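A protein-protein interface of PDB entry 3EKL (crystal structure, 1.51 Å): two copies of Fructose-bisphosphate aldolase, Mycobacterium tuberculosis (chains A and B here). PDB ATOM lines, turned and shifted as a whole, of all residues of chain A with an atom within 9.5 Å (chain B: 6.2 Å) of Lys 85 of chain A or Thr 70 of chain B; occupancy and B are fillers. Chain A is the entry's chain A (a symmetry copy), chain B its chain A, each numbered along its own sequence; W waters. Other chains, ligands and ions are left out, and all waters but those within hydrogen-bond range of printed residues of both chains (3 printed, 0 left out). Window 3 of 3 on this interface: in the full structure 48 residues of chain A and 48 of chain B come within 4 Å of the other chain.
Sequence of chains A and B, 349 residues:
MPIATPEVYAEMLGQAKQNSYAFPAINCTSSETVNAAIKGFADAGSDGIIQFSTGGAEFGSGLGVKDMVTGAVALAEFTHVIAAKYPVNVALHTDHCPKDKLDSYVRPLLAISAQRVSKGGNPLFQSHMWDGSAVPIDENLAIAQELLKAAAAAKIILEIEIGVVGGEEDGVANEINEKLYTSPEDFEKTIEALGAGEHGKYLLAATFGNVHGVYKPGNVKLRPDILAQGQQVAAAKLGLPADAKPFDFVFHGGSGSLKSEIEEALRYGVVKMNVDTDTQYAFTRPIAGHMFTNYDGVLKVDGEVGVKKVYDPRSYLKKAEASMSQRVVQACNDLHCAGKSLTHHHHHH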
ATOM      1  N   PRO A   2      30.200  35.773  23.478  1.00  0.00           N
ATOM      2  CA  PRO A   2      29.219  36.462  24.337  1.00  0.00           C
ATOM      3  C   PRO A   2      27.861  36.574  23.652  1.00  0.00           C
ATOM      4  O   PRO A   2      27.765  36.392  22.438  1.00  0.00           O
ATOM      5  CB  PRO A   2      29.830  37.860  24.504  1.00  0.00           C
ATOM      6  CG  PRO A   2      30.744  38.017  23.306  1.00  0.00           C
ATOM      7  CD  PRO A   2      31.323  36.657  23.119  1.00  0.00           C
ATOM      8  N   ILE A   3      26.805  36.862  24.416  1.00  0.00           N
ATOM      9  CA  ILE A   3      25.555  37.315  23.799  1.00  0.00           C
ATOM     10  C   ILE A   3      25.855  38.613  23.034  1.00  0.00           C
ATOM     11  O   ILE A   3      26.600  39.476  23.515  1.00  0.00           O
ATOM     12  CB  ILE A   3      24.452  37.580  24.859  1.00  0.00           C
ATOM     13  CG1 ILE A   3      24.034  36.273  25.537  1.00  0.00           C
ATOM     14  CG2 ILE A   3      23.230  38.280  24.238  1.00  0.00           C
ATOM     15  CD1 ILE A   3      23.311  35.273  24.632  1.00  0.00           C
ATOM     16  N   ASN A  35      23.088  24.469  22.853  1.00  0.00           N
ATOM     17  CA  ASN A  35      24.511  24.141  22.943  1.00  0.00           C
ATOM     18  C   ASN A  35      25.064  23.744  21.580  1.00  0.00           C
ATOM     19  O   ASN A  35      26.186  24.141  21.203  1.00  0.00           O
ATOM     20  CB  ASN A  35      24.747  23.045  23.987  1.00  0.00           C
ATOM     21  CG  ASN A  35      24.784  23.597  25.398  1.00  0.00           C
ATOM     22  OD1 ASN A  35      25.085  24.765  25.599  1.00  0.00           O
ATOM     23  ND2 ASN A  35      24.489  22.751  26.382  1.00  0.00           N
ATOM     24  N   ILE A  38      25.342  26.998  19.244  1.00  0.00           N
ATOM     25  CA  ILE A  38      26.475  27.875  19.582  1.00  0.00           C
ATOM     26  C   ILE A  38      27.836  27.224  19.260  1.00  0.00           C
ATOM     27  O   ILE A  38      28.730  27.876  18.713  1.00  0.00           O
ATOM     28  CB  ILE A  38      26.433  28.353  21.054  1.00  0.00           C
ATOM     29  CG1 ILE A  38      25.130  29.100  21.315  1.00  0.00           C
ATOM     30  CG2 ILE A  38      27.625  29.280  21.332  1.00  0.00           C
ATOM     31  CD1 ILE A  38      24.920  29.490  22.775  1.00  0.00           C
ATOM     32  N   LYS A  39      27.990  25.934  19.565  1.00  0.00           N
ATOM     33  CA  LYS A  39      29.242  25.230  19.226  1.00  0.00           C
ATOM     34  C   LYS A  39      29.457  25.232  17.703  1.00  0.00           C
ATOM     35  O   LYS A  39      30.586  25.356  17.240  1.00  0.00           O
ATOM     36  CB  LYS A  39      29.224  23.808  19.806  1.00  0.00           C
ATOM     37  CG  LYS A  39      30.363  22.876  19.387  1.00  0.00           C
ATOM     38  CD  LYS A  39      31.739  23.423  19.717  1.00  0.00           C
ATOM     39  CE  LYS A  39      32.739  22.274  19.955  1.00  0.00           C
ATOM     40  NZ  LYS A  39      32.802  21.300  18.814  1.00  0.00           N
ATOM     41  N   ALA A  42      30.769  28.647  16.787  1.00  0.00           N
ATOM     42  CA  ALA A  42      32.149  28.776  17.252  1.00  0.00           C
ATOM     43  C   ALA A  42      33.098  27.964  16.385  1.00  0.00           C
ATOM     44  O   ALA A  42      34.178  28.437  16.012  1.00  0.00           O
ATOM     45  CB  ALA A  42      32.265  28.374  18.720  1.00  0.00           C
ATOM     46  N   GLU A  77      17.658  32.694  29.388  1.00  0.00           N
ATOM     47  CA  GLU A  77      18.555  32.817  30.549  1.00  0.00           C
ATOM     48  C   GLU A  77      19.647  31.751  30.504  1.00  0.00           C
ATOM     49  O   GLU A  77      20.813  32.042  30.764  1.00  0.00           O
ATOM     50  CB  GLU A  77      17.787  32.760  31.877  1.00  0.00           C
ATOM     51  CG  GLU A  77      16.808  33.912  32.095  1.00  0.00           C
ATOM     52  CD  GLU A  77      17.468  35.275  32.281  1.00  0.00           C
ATOM     53  OE1 GLU A  77      16.727  36.251  32.559  1.00  0.00           O
ATOM     54  OE2 GLU A  77      18.710  35.403  32.142  1.00  0.00           O
ATOM     55  N   PHE A  78      19.273  30.524  30.137  1.00  0.00           N
ATOM     56  CA  PHE A  78      20.250  29.472  29.926  1.00  0.00           C
ATOM     57  C   PHE A  78      21.286  29.922  28.889  1.00  0.00           C
ATOM     58  O   PHE A  78      22.497  29.797  29.109  1.00  0.00           O
ATOM     59  CB  PHE A  78      19.531  28.208  29.455  1.00  0.00           C
ATOM     60  CG  PHE A  78      20.467  27.106  29.065  1.00  0.00           C
ATOM     61  CD1 PHE A  78      20.935  26.190  30.010  1.00  0.00           C
ATOM     62  CD2 PHE A  78      20.903  26.980  27.738  1.00  0.00           C
ATOM     63  CE1 PHE A  78      21.820  25.181  29.646  1.00  0.00           C
ATOM     64  CE2 PHE A  78      21.793  25.981  27.374  1.00  0.00           C
ATOM     65  CZ  PHE A  78      22.255  25.081  28.322  1.00  0.00           C
ATOM     66  N   THR A  79      20.796  30.425  27.754  1.00  0.00           N
ATOM     67  CA  THR A  79      21.686  30.827  26.655  1.00  0.00           C
ATOM     68  C   THR A  79      22.635  31.963  27.062  1.00  0.00           C
ATOM     69  O   THR A  79      23.797  31.981  26.621  1.00  0.00           O
ATOM     70  CB  THR A  79      20.858  31.233  25.425  1.00  0.00           C
ATOM     71  OG1 THR A  79      19.990  30.153  25.069  1.00  0.00           O
ATOM     72  CG2 THR A  79      21.760  31.566  24.245  1.00  0.00           C
ATOM     73  N   HIS A  80      22.161  32.903  27.889  1.00  0.00           N
ATOM     74  CA  HIS A  80      23.062  33.975  28.354  1.00  0.00           C
ATOM     75  C   HIS A  80      24.277  33.429  29.103  1.00  0.00           C
ATOM     76  O   HIS A  80      25.386  33.931  28.929  1.00  0.00           O
ATOM     77  CB  HIS A  80      22.333  35.011  29.216  1.00  0.00           C
ATOM     78  CG  HIS A  80      21.559  36.020  28.424  1.00  0.00           C
ATOM     79  ND1 HIS A  80      21.908  37.354  28.363  1.00  0.00           N
ATOM     80  CD2 HIS A  80      20.463  35.881  27.640  1.00  0.00           C
ATOM     81  CE1 HIS A  80      21.047  37.996  27.588  1.00  0.00           C
ATOM     82  NE2 HIS A  80      20.163  37.125  27.133  1.00  0.00           N
ATOM     83  N   VAL A  81      24.071  32.411  29.935  1.00  0.00           N
ATOM     84  CA  VAL A  81      25.177  31.841  30.692  1.00  0.00           C
ATOM     85  C   VAL A  81      26.143  31.123  29.751  1.00  0.00           C
ATOM     86  O   VAL A  81      27.362  31.284  29.853  1.00  0.00           O
ATOM     87  CB  VAL A  81      24.664  30.888  31.797  1.00  0.00           C
ATOM     88  CG1 VAL A  81      25.815  30.202  32.522  1.00  0.00           C
ATOM     89  CG2 VAL A  81      23.800  31.656  32.788  1.00  0.00           C
ATOM     90  N   ILE A  82      25.595  30.326  28.837  1.00  0.00           N
ATOM     91  CA  ILE A  82      26.442  29.557  27.916  1.00  0.00           C
ATOM     92  C   ILE A  82      27.240  30.457  26.969  1.00  0.00           C
ATOM     93  O   ILE A  82      28.462  30.278  26.801  1.00  0.00           O
ATOM     94  CB  ILE A  82      25.604  28.568  27.082  1.00  0.00           C
ATOM     95  CG1 ILE A  82      24.880  27.586  28.017  1.00  0.00           C
ATOM     96  CG2 ILE A  82      26.484  27.845  26.054  1.00  0.00           C
ATOM     97  CD1 ILE A  82      25.798  26.720  28.885  1.00  0.00           C
ATOM     98  N   ALA A  83      26.553  31.424  26.352  1.00  0.00           N
ATOM     99  CA  ALA A  83      27.203  32.232  25.304  1.00  0.00           C
ATOM    100  C   ALA A  83      28.377  33.040  25.837  1.00  0.00           C
ATOM    101  O   ALA A  83      29.301  33.365  25.079  1.00  0.00           O
ATOM    102  CB  ALA A  83      26.204  33.145  24.630  1.00  0.00           C
ATOM    103  N   ALA A  84      28.359  33.349  27.132  1.00  0.00           N
ATOM    104  CA  ALA A  84      29.469  34.089  27.750  1.00  0.00           C
ATOM    105  C   ALA A  84      30.799  33.326  27.678  1.00  0.00           C
ATOM    106  O   ALA A  84      31.871  33.924  27.811  1.00  0.00           O
ATOM    107  CB  ALA A  84      29.141  34.447  29.204  1.00  0.00           C
ATOM    108  N   LYS A  85      30.725  32.009  27.462  1.00  0.00           N
ATOM    109  CA  LYS A  85      31.911  31.156  27.436  1.00  0.00           C
ATOM    110  C   LYS A  85      32.457  30.901  26.025  1.00  0.00           C
ATOM    111  O   LYS A  85      33.402  30.131  25.848  1.00  0.00           O
ATOM    112  CB  LYS A  85      31.604  29.828  28.137  1.00  0.00           C
ATOM    113  CG  LYS A  85      31.213  29.980  29.602  1.00  0.00           C
ATOM    114  CD  LYS A  85      32.316  30.567  30.450  1.00  0.00           C
ATOM    115  CE  LYS A  85      33.392  29.542  30.769  1.00  0.00           C
ATOM    116  NZ  LYS A  85      34.400  30.102  31.714  1.00  0.00           N
ATOM    117  N   TYR A  86      31.867  31.554  25.026  1.00  0.00           N
ATOM    118  CA  TYR A  86      32.323  31.406  23.645  1.00  0.00           C
ATOM    119  C   TYR A  86      32.806  32.737  23.071  1.00  0.00           C
ATOM    120  O   TYR A  86      32.225  33.787  23.381  1.00  0.00           O
ATOM    121  CB  TYR A  86      31.183  30.917  22.772  1.00  0.00           C
ATOM    122  CG  TYR A  86      30.819  29.463  22.927  1.00  0.00           C
ATOM    123  CD1 TYR A  86      31.426  28.487  22.141  1.00  0.00           C
ATOM    124  CD2 TYR A  86      29.835  29.069  23.833  1.00  0.00           C
ATOM    125  CE1 TYR A  86      31.073  27.149  22.232  1.00  0.00           C
ATOM    126  CE2 TYR A  86      29.466  27.733  23.936  1.00  0.00           C
ATOM    127  CZ  TYR A  86      30.091  26.780  23.135  1.00  0.00           C
ATOM    128  OH  TYR A  86      29.729  25.455  23.214  1.00  0.00           O
ATOM    129  N   PRO A  87      33.840  32.700  22.224  1.00  0.00           N
ATOM    130  CA  PRO A  87      34.389  33.959  21.713  1.00  0.00           C
ATOM    131  C   PRO A  87      33.503  34.700  20.707  1.00  0.00           C
ATOM    132  O   PRO A  87      33.715  35.894  20.495  1.00  0.00           O
ATOM    133  CB  PRO A  87      35.706  33.523  21.059  1.00  0.00           C
ATOM    134  CG  PRO A  87      35.490  32.100  20.680  1.00  0.00           C
ATOM    135  CD  PRO A  87      34.578  31.523  21.723  1.00  0.00           C
ATOM    136  N   VAL A  88      32.520  34.011  20.124  1.00  0.00           N
ATOM    137  CA  VAL A  88      31.713  34.533  19.007  1.00  0.00           C
ATOM    138  C   VAL A  88      30.475  35.219  19.571  1.00  0.00           C
ATOM    139  O   VAL A  88      30.127  34.992  20.739  1.00  0.00           O
ATOM    140  CB  VAL A  88      31.299  33.419  18.011  1.00  0.00           C
ATOM    141  CG1 VAL A  88      32.539  32.822  17.343  1.00  0.00           C
ATOM    142  CG2 VAL A  88      30.436  32.349  18.700  1.00  0.00           C
ATOM    143  N   ASN A  89      29.808  36.037  18.754  1.00  0.00           N
ATOM    144  CA  ASN A  89      28.604  36.745  19.194  1.00  0.00           C
ATOM    145  C   ASN A  89      27.365  35.968  18.831  1.00  0.00           C
ATOM    146  O   ASN A  89      27.197  35.548  17.675  1.00  0.00           O
ATOM    147  CB  ASN A  89      28.527  38.130  18.549  1.00  0.00           C
ATOM    148  CG  ASN A  89      29.716  38.981  18.888  1.00  0.00           C
ATOM    149  OD1 ASN A  89      29.916  39.373  20.046  1.00  0.00           O
ATOM    150  ND2 ASN A  89      30.521  39.288  17.872  1.00  0.00           N
ATOM    151  N   VAL A  90      26.497  35.797  19.827  1.00  0.00           N
ATOM    152  CA  VAL A  90      25.267  35.021  19.689  1.00  0.00           C
ATOM    153  C   VAL A  90      24.071  35.923  19.977  1.00  0.00           C
ATOM    154  O   VAL A  90      23.937  36.435  21.090  1.00  0.00           O
ATOM    155  CB  VAL A  90      25.273  33.825  20.682  1.00  0.00           C
ATOM    156  CG1 VAL A  90      23.983  33.029  20.584  1.00  0.00           C
ATOM    157  CG2 VAL A  90      26.482  32.923  20.437  1.00  0.00           C
ATOM    158  N   HIS A 345      38.643  36.154  16.333  1.00  0.00           N
ATOM    159  CA  HIS A 345      39.436  35.070  16.923  1.00  0.00           C
ATOM    160  C   HIS A 345      39.815  34.051  15.852  1.00  0.00           C
ATOM    161  O   HIS A 345      39.083  33.081  15.617  1.00  0.00           O
ATOM    162  CB  HIS A 345      38.640  34.355  18.024  1.00  0.00           C
ATOM    163  CG  HIS A 345      38.810  34.944  19.387  1.00  0.00           C
ATOM    164  ND1 HIS A 345      39.910  34.687  20.174  1.00  0.00           N
ATOM    165  CD2 HIS A 345      38.007  35.758  20.115  1.00  0.00           C
ATOM    166  CE1 HIS A 345      39.786  35.323  21.325  1.00  0.00           C
ATOM    167  NE2 HIS A 345      38.640  35.981  21.315  1.00  0.00           N
ATOM    168  N   ALA B  57      26.588  18.379  34.977  1.00  0.00           N
ATOM    169  CA  ALA B  57      26.902  19.801  34.783  1.00  0.00           C
ATOM    170  C   ALA B  57      27.816  20.022  33.562  1.00  0.00           C
ATOM    171  O   ALA B  57      27.570  20.927  32.752  1.00  0.00           O
ATOM    172  CB  ALA B  57      27.547  20.372  36.050  1.00  0.00           C
ATOM    173  N   GLY B  60      25.688  19.643  30.624  1.00  0.00           N
ATOM    174  CA  GLY B  60      24.802  20.813  30.513  1.00  0.00           C
ATOM    175  C   GLY B  60      25.486  22.023  29.904  1.00  0.00           C
ATOM    176  O   GLY B  60      24.822  22.877  29.298  1.00  0.00           O
ATOM    177  N   SER B  61      26.809  22.114  30.069  1.00  0.00           N
ATOM    178  CA  SER B  61      27.564  23.266  29.560  1.00  0.00           C
ATOM    179  C   SER B  61      27.863  23.149  28.066  1.00  0.00           C
ATOM    180  O   SER B  61      28.312  24.131  27.464  1.00  0.00           O
ATOM    181  CB  SER B  61      28.880  23.436  30.331  1.00  0.00           C
ATOM    182  OG  SER B  61      29.843  22.463  29.948  1.00  0.00           O
ATOM    183  N   GLY B  64      31.274  22.262  23.654  1.00  0.00           N
ATOM    184  CA  GLY B  64      32.147  23.388  23.349  1.00  0.00           C
ATOM    185  C   GLY B  64      32.706  24.102  24.564  1.00  0.00           C
ATOM    186  O   GLY B  64      33.563  24.981  24.434  1.00  0.00           O
ATOM    187  N   VAL B  65      32.227  23.712  25.747  1.00  0.00           N
ATOM    188  CA  VAL B  65      32.609  24.372  26.997  1.00  0.00           C
ATOM    189  C   VAL B  65      33.175  23.378  28.015  1.00  0.00           C
ATOM    190  O   VAL B  65      34.282  23.577  28.530  1.00  0.00           O
ATOM    191  CB  VAL B  65      31.423  25.154  27.623  1.00  0.00           C
ATOM    192  CG1 VAL B  65      31.866  25.860  28.893  1.00  0.00           C
ATOM    193  CG2 VAL B  65      30.854  26.187  26.647  1.00  0.00           C
ATOM    194  N   ASP B  67      32.491  22.741  31.171  1.00  0.00           N
ATOM    195  CA  ASP B  67      32.817  23.396  32.431  1.00  0.00           C
ATOM    196  C   ASP B  67      31.681  23.177  33.416  1.00  0.00           C
ATOM    197  O   ASP B  67      30.532  23.551  33.153  1.00  0.00           O
ATOM    198  CB  ASP B  67      33.045  24.892  32.231  1.00  0.00           C
ATOM    199  CG  ASP B  67      33.478  25.581  33.507  1.00  0.00           C
ATOM    200  OD1 ASP B  67      34.604  25.316  33.978  1.00  0.00           O
ATOM    201  OD2 ASP B  67      32.676  26.357  34.060  1.00  0.00           O
ATOM    202  N   MET B  68      32.017  22.583  34.556  1.00  0.00           N
ATOM    203  CA  MET B  68      31.013  22.216  35.552  1.00  0.00           C
ATOM    204  C   MET B  68      30.254  23.416  36.107  1.00  0.00           C
ATOM    205  O   MET B  68      29.031  23.372  36.245  1.00  0.00           O
ATOM    206  CB  MET B  68      31.656  21.458  36.715  1.00  0.00           C
ATOM    207  CG  MET B  68      32.216  20.116  36.333  1.00  0.00           C
ATOM    208  SD  MET B  68      33.074  19.348  37.722  1.00  0.00           S
ATOM    209  CE  MET B  68      34.559  20.332  37.787  1.00  0.00           C
ATOM    210  N   VAL B  69      30.981  24.478  36.457  1.00  0.00           N
ATOM    211  CA  VAL B  69      30.294  25.647  37.024  1.00  0.00           C
ATOM    212  C   VAL B  69      29.324  26.238  35.993  1.00  0.00           C
ATOM    213  O   VAL B  69      28.168  26.517  36.310  1.00  0.00           O
ATOM    214  CB  VAL B  69      31.290  26.704  37.527  1.00  0.00           C
ATOM    215  CG1 VAL B  69      30.587  28.026  37.819  1.00  0.00           C
ATOM    216  CG2 VAL B  69      31.999  26.181  38.785  1.00  0.00           C
ATOM    217  N   THR B  70      29.785  26.396  34.753  1.00  0.00           N
ATOM    218  CA  THR B  70      28.934  26.970  33.714  1.00  0.00           C
ATOM    219  C   THR B  70      27.656  26.145  33.527  1.00  0.00           C
ATOM    220  O   THR B  70      26.550  26.701  33.439  1.00  0.00           O
ATOM    221  CB  THR B  70      29.678  27.066  32.381  1.00  0.00           C
ATOM    222  OG1 THR B  70      30.846  27.858  32.557  1.00  0.00           O
ATOM    223  CG2 THR B  70      28.795  27.700  31.297  1.00  0.00           C
ATOM    224  N   GLY B  71      27.800  24.816  33.465  1.00  0.00           N
ATOM    225  CA  GLY B  71      26.631  23.957  33.256  1.00  0.00           C
ATOM    226  C   GLY B  71      25.659  24.001  34.419  1.00  0.00           C
ATOM    227  O   GLY B  71      24.441  24.068  34.223  1.00  0.00           O
ATOM    228  N   ALA B  72      26.200  23.972  35.639  1.00  0.00           N
ATOM    229  CA  ALA B  72      25.346  24.044  36.822  1.00  0.00           C
ATOM    230  C   ALA B  72      24.616  25.391  36.937  1.00  0.00           C
ATOM    231  O   ALA B  72      23.419  25.433  37.266  1.00  0.00           O
ATOM    232  CB  ALA B  72      26.161  23.752  38.092  1.00  0.00           C
ATOM    233  N   VAL B  73      25.326  26.487  36.668  1.00  0.00           N
ATOM    234  CA  VAL B  73      24.694  27.808  36.715  1.00  0.00           C
ATOM    235  C   VAL B  73      23.634  27.946  35.622  1.00  0.00           C
ATOM    236  O   VAL B  73      22.521  28.411  35.890  1.00  0.00           O
ATOM    237  CB  VAL B  73      25.740  28.944  36.629  1.00  0.00           C
ATOM    238  CG1 VAL B  73      25.052  30.290  36.493  1.00  0.00           C
ATOM    239  CG2 VAL B  73      26.651  28.928  37.859  1.00  0.00           C
ATOM    240  N   ALA B  74      23.967  27.528  34.407  1.00  0.00           N
ATOM    241  CA  ALA B  74      23.022  27.662  33.301  1.00  0.00           C
ATOM    242  C   ALA B  74      21.748  26.854  33.571  1.00  0.00           C
ATOM    243  O   ALA B  74      20.621  27.350  33.383  1.00  0.00           O
ATOM    244  CB  ALA B  74      23.673  27.221  31.998  1.00  0.00           C
ATOM    245  N   LEU B  75      21.921  25.609  34.014  1.00  0.00           N
ATOM    246  CA  LEU B  75      20.760  24.780  34.328  1.00  0.00           C
ATOM    247  C   LEU B  75      20.001  25.300  35.545  1.00  0.00           C
ATOM    248  O   LEU B  75      18.765  25.249  35.575  1.00  0.00           O
ATOM    249  CB  LEU B  75      21.150  23.304  34.507  1.00  0.00           C
ATOM    250  CG  LEU B  75      21.600  22.559  33.243  1.00  0.00           C
ATOM    251  CD1 LEU B  75      22.154  21.198  33.636  1.00  0.00           C
ATOM    252  CD2 LEU B  75      20.479  22.432  32.224  1.00  0.00           C
HETATM  253  O   HOH W   1      34.165  27.603  25.089  1.00  0.00           O
HETATM  254  O   HOH W   2      27.786  25.008  24.964  1.00  0.00           O
HETATM  255  O   HOH W   3      28.404  22.824  23.021  1.00  0.00           O
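Printed residues of chain B that touch a printed residue of chain A: Gly 60, Ser 61, Gly 64, Val 65, Thr 70 and Ala 74.
Hydrophobic or aromatic side chains of chain B within 4 Å of the printed part of chain A: Val 65 and Ala 74.
Of the 21 printed residues of chain A, 7 touch a printed residue of chain B.
Hydrophobic or aromatic side chains of chain A that line the printed part of chain B: Phe 78, Val 81, Ile 82 and Tyr 86.
Among the printed residues, 14 pairs touch across the chains.
Water W2 lies within hydrogen-bond range of the side-chain hydroxyl of Tyr 86 of chain A (2.7 Å), the backbone carbonyl oxygen of Ser 61 of chain B (2.7 Å) and the side-chain amide oxygen of Asn 35 of chain A (2.8 Å).
Water W1 bridges O of Lys 85 of chain A (2.7 Å) and O of Gly 64 of chain B (2.8 Å).
Water W3 lies within hydrogen-bond range of the side-chain hydroxyl (OH) of Tyr 86 of chain A (3.0 Å), the backbone NH (N) of Gly 64 of chain B (3.0 Å) and the backbone carbonyl oxygen (O) of Asn 35 of chain A (3.2 Å).
The backbone carbonyl oxygen (O) of Gly 60 of chain B is in hydrogen-bond range of the side-chain amide nitrogen (ND2) of Asn 35 of chain A, at 2.9 Å.
OG of Ser 61 of chain B sits at hydrogen-bond distance from N of Asp 67 of chain B (2.9 Å).
OD2 of Asp 67 of chain B is in hydrogen-bond range of OG1 of Thr 70 of chain B, at 2.8 Å.
Printed residues of chain B within 4 Å of Phe 78 of chain A: Gly 60 (3.5 Å) and Ala 74 (3.5 Å).
Thr 79 of chain A touches none of the printed residues of chain B.
Of the printed residues of chain B, Ile 82 of chain A touches Gly 60, Ser 61, Thr 70 and Ala 74.
Ala 83 of chain A touches none of the printed residues of chain B.
Of the printed residues of chain B, Lys 85 of chain A touches Thr 70 (3.5 Å).
Of the printed residues of chain A, Gly 64 of chain B touches Lys 39 and Tyr 86.
Of the printed residues of chain A, Val 65 of chain B touches Tyr 86.
No residue of chain A comes within 4 Å of Asp 67 of chain B.
Of the printed residues of chain A, Thr 70 of chain B touches Val 81 (3.7 Å), Ile 82 (3.97 Å) and Lys 85 (3.5 Å).
Gly 71 of chain B touches none of the printed residues of chain A.
No residue of chain A comes within 4 Å of Ala 72 of chain B.
Printed residues of chain A within 4 Å of Ala 74 of chain B: Phe 78, Val 81 and Ile 82.
The nearest residue of chain A that does not touch Thr 70 of chain B is Phe 78 of chain A (6.3 Å).
OD1 of Asn 35 of chain A touches O of Ser 61 of chain B, 3.8 Å away.
CZ of Phe 78 of chain A touches O of Gly 60 of chain B (3.5 Å).
Ala 74 of chain B touches Phe 78 of chain A (CB to CD1, 3.5 Å).
O of Thr 70 of chain B touches CG1 of Val 81 of chain A, at 3.7 Å.
Ile 82 of chain A touches Gly 60 of chain B.
Ile 82 of chain A touches Ser 61 of chain B.
Thr 70 of chain B touches Ile 82 of chain A (CG2 to CD1, 3.97 Å).
CD1 of Ile 82 of chain A touches CB of Ala 74 of chain B, at 3.8 Å.
OG1 of Thr 70 of chain B touches CE of Lys 85 of chain A, at 3.5 Å.
OH of Tyr 86 of chain A touches CA of Gly 64 of chain B, at 3.2 Å.
No position is printed for both chains.
Of the 14 pairs that touch across the chains among the printed residues, none has its exchanged pair printed and touching as well.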
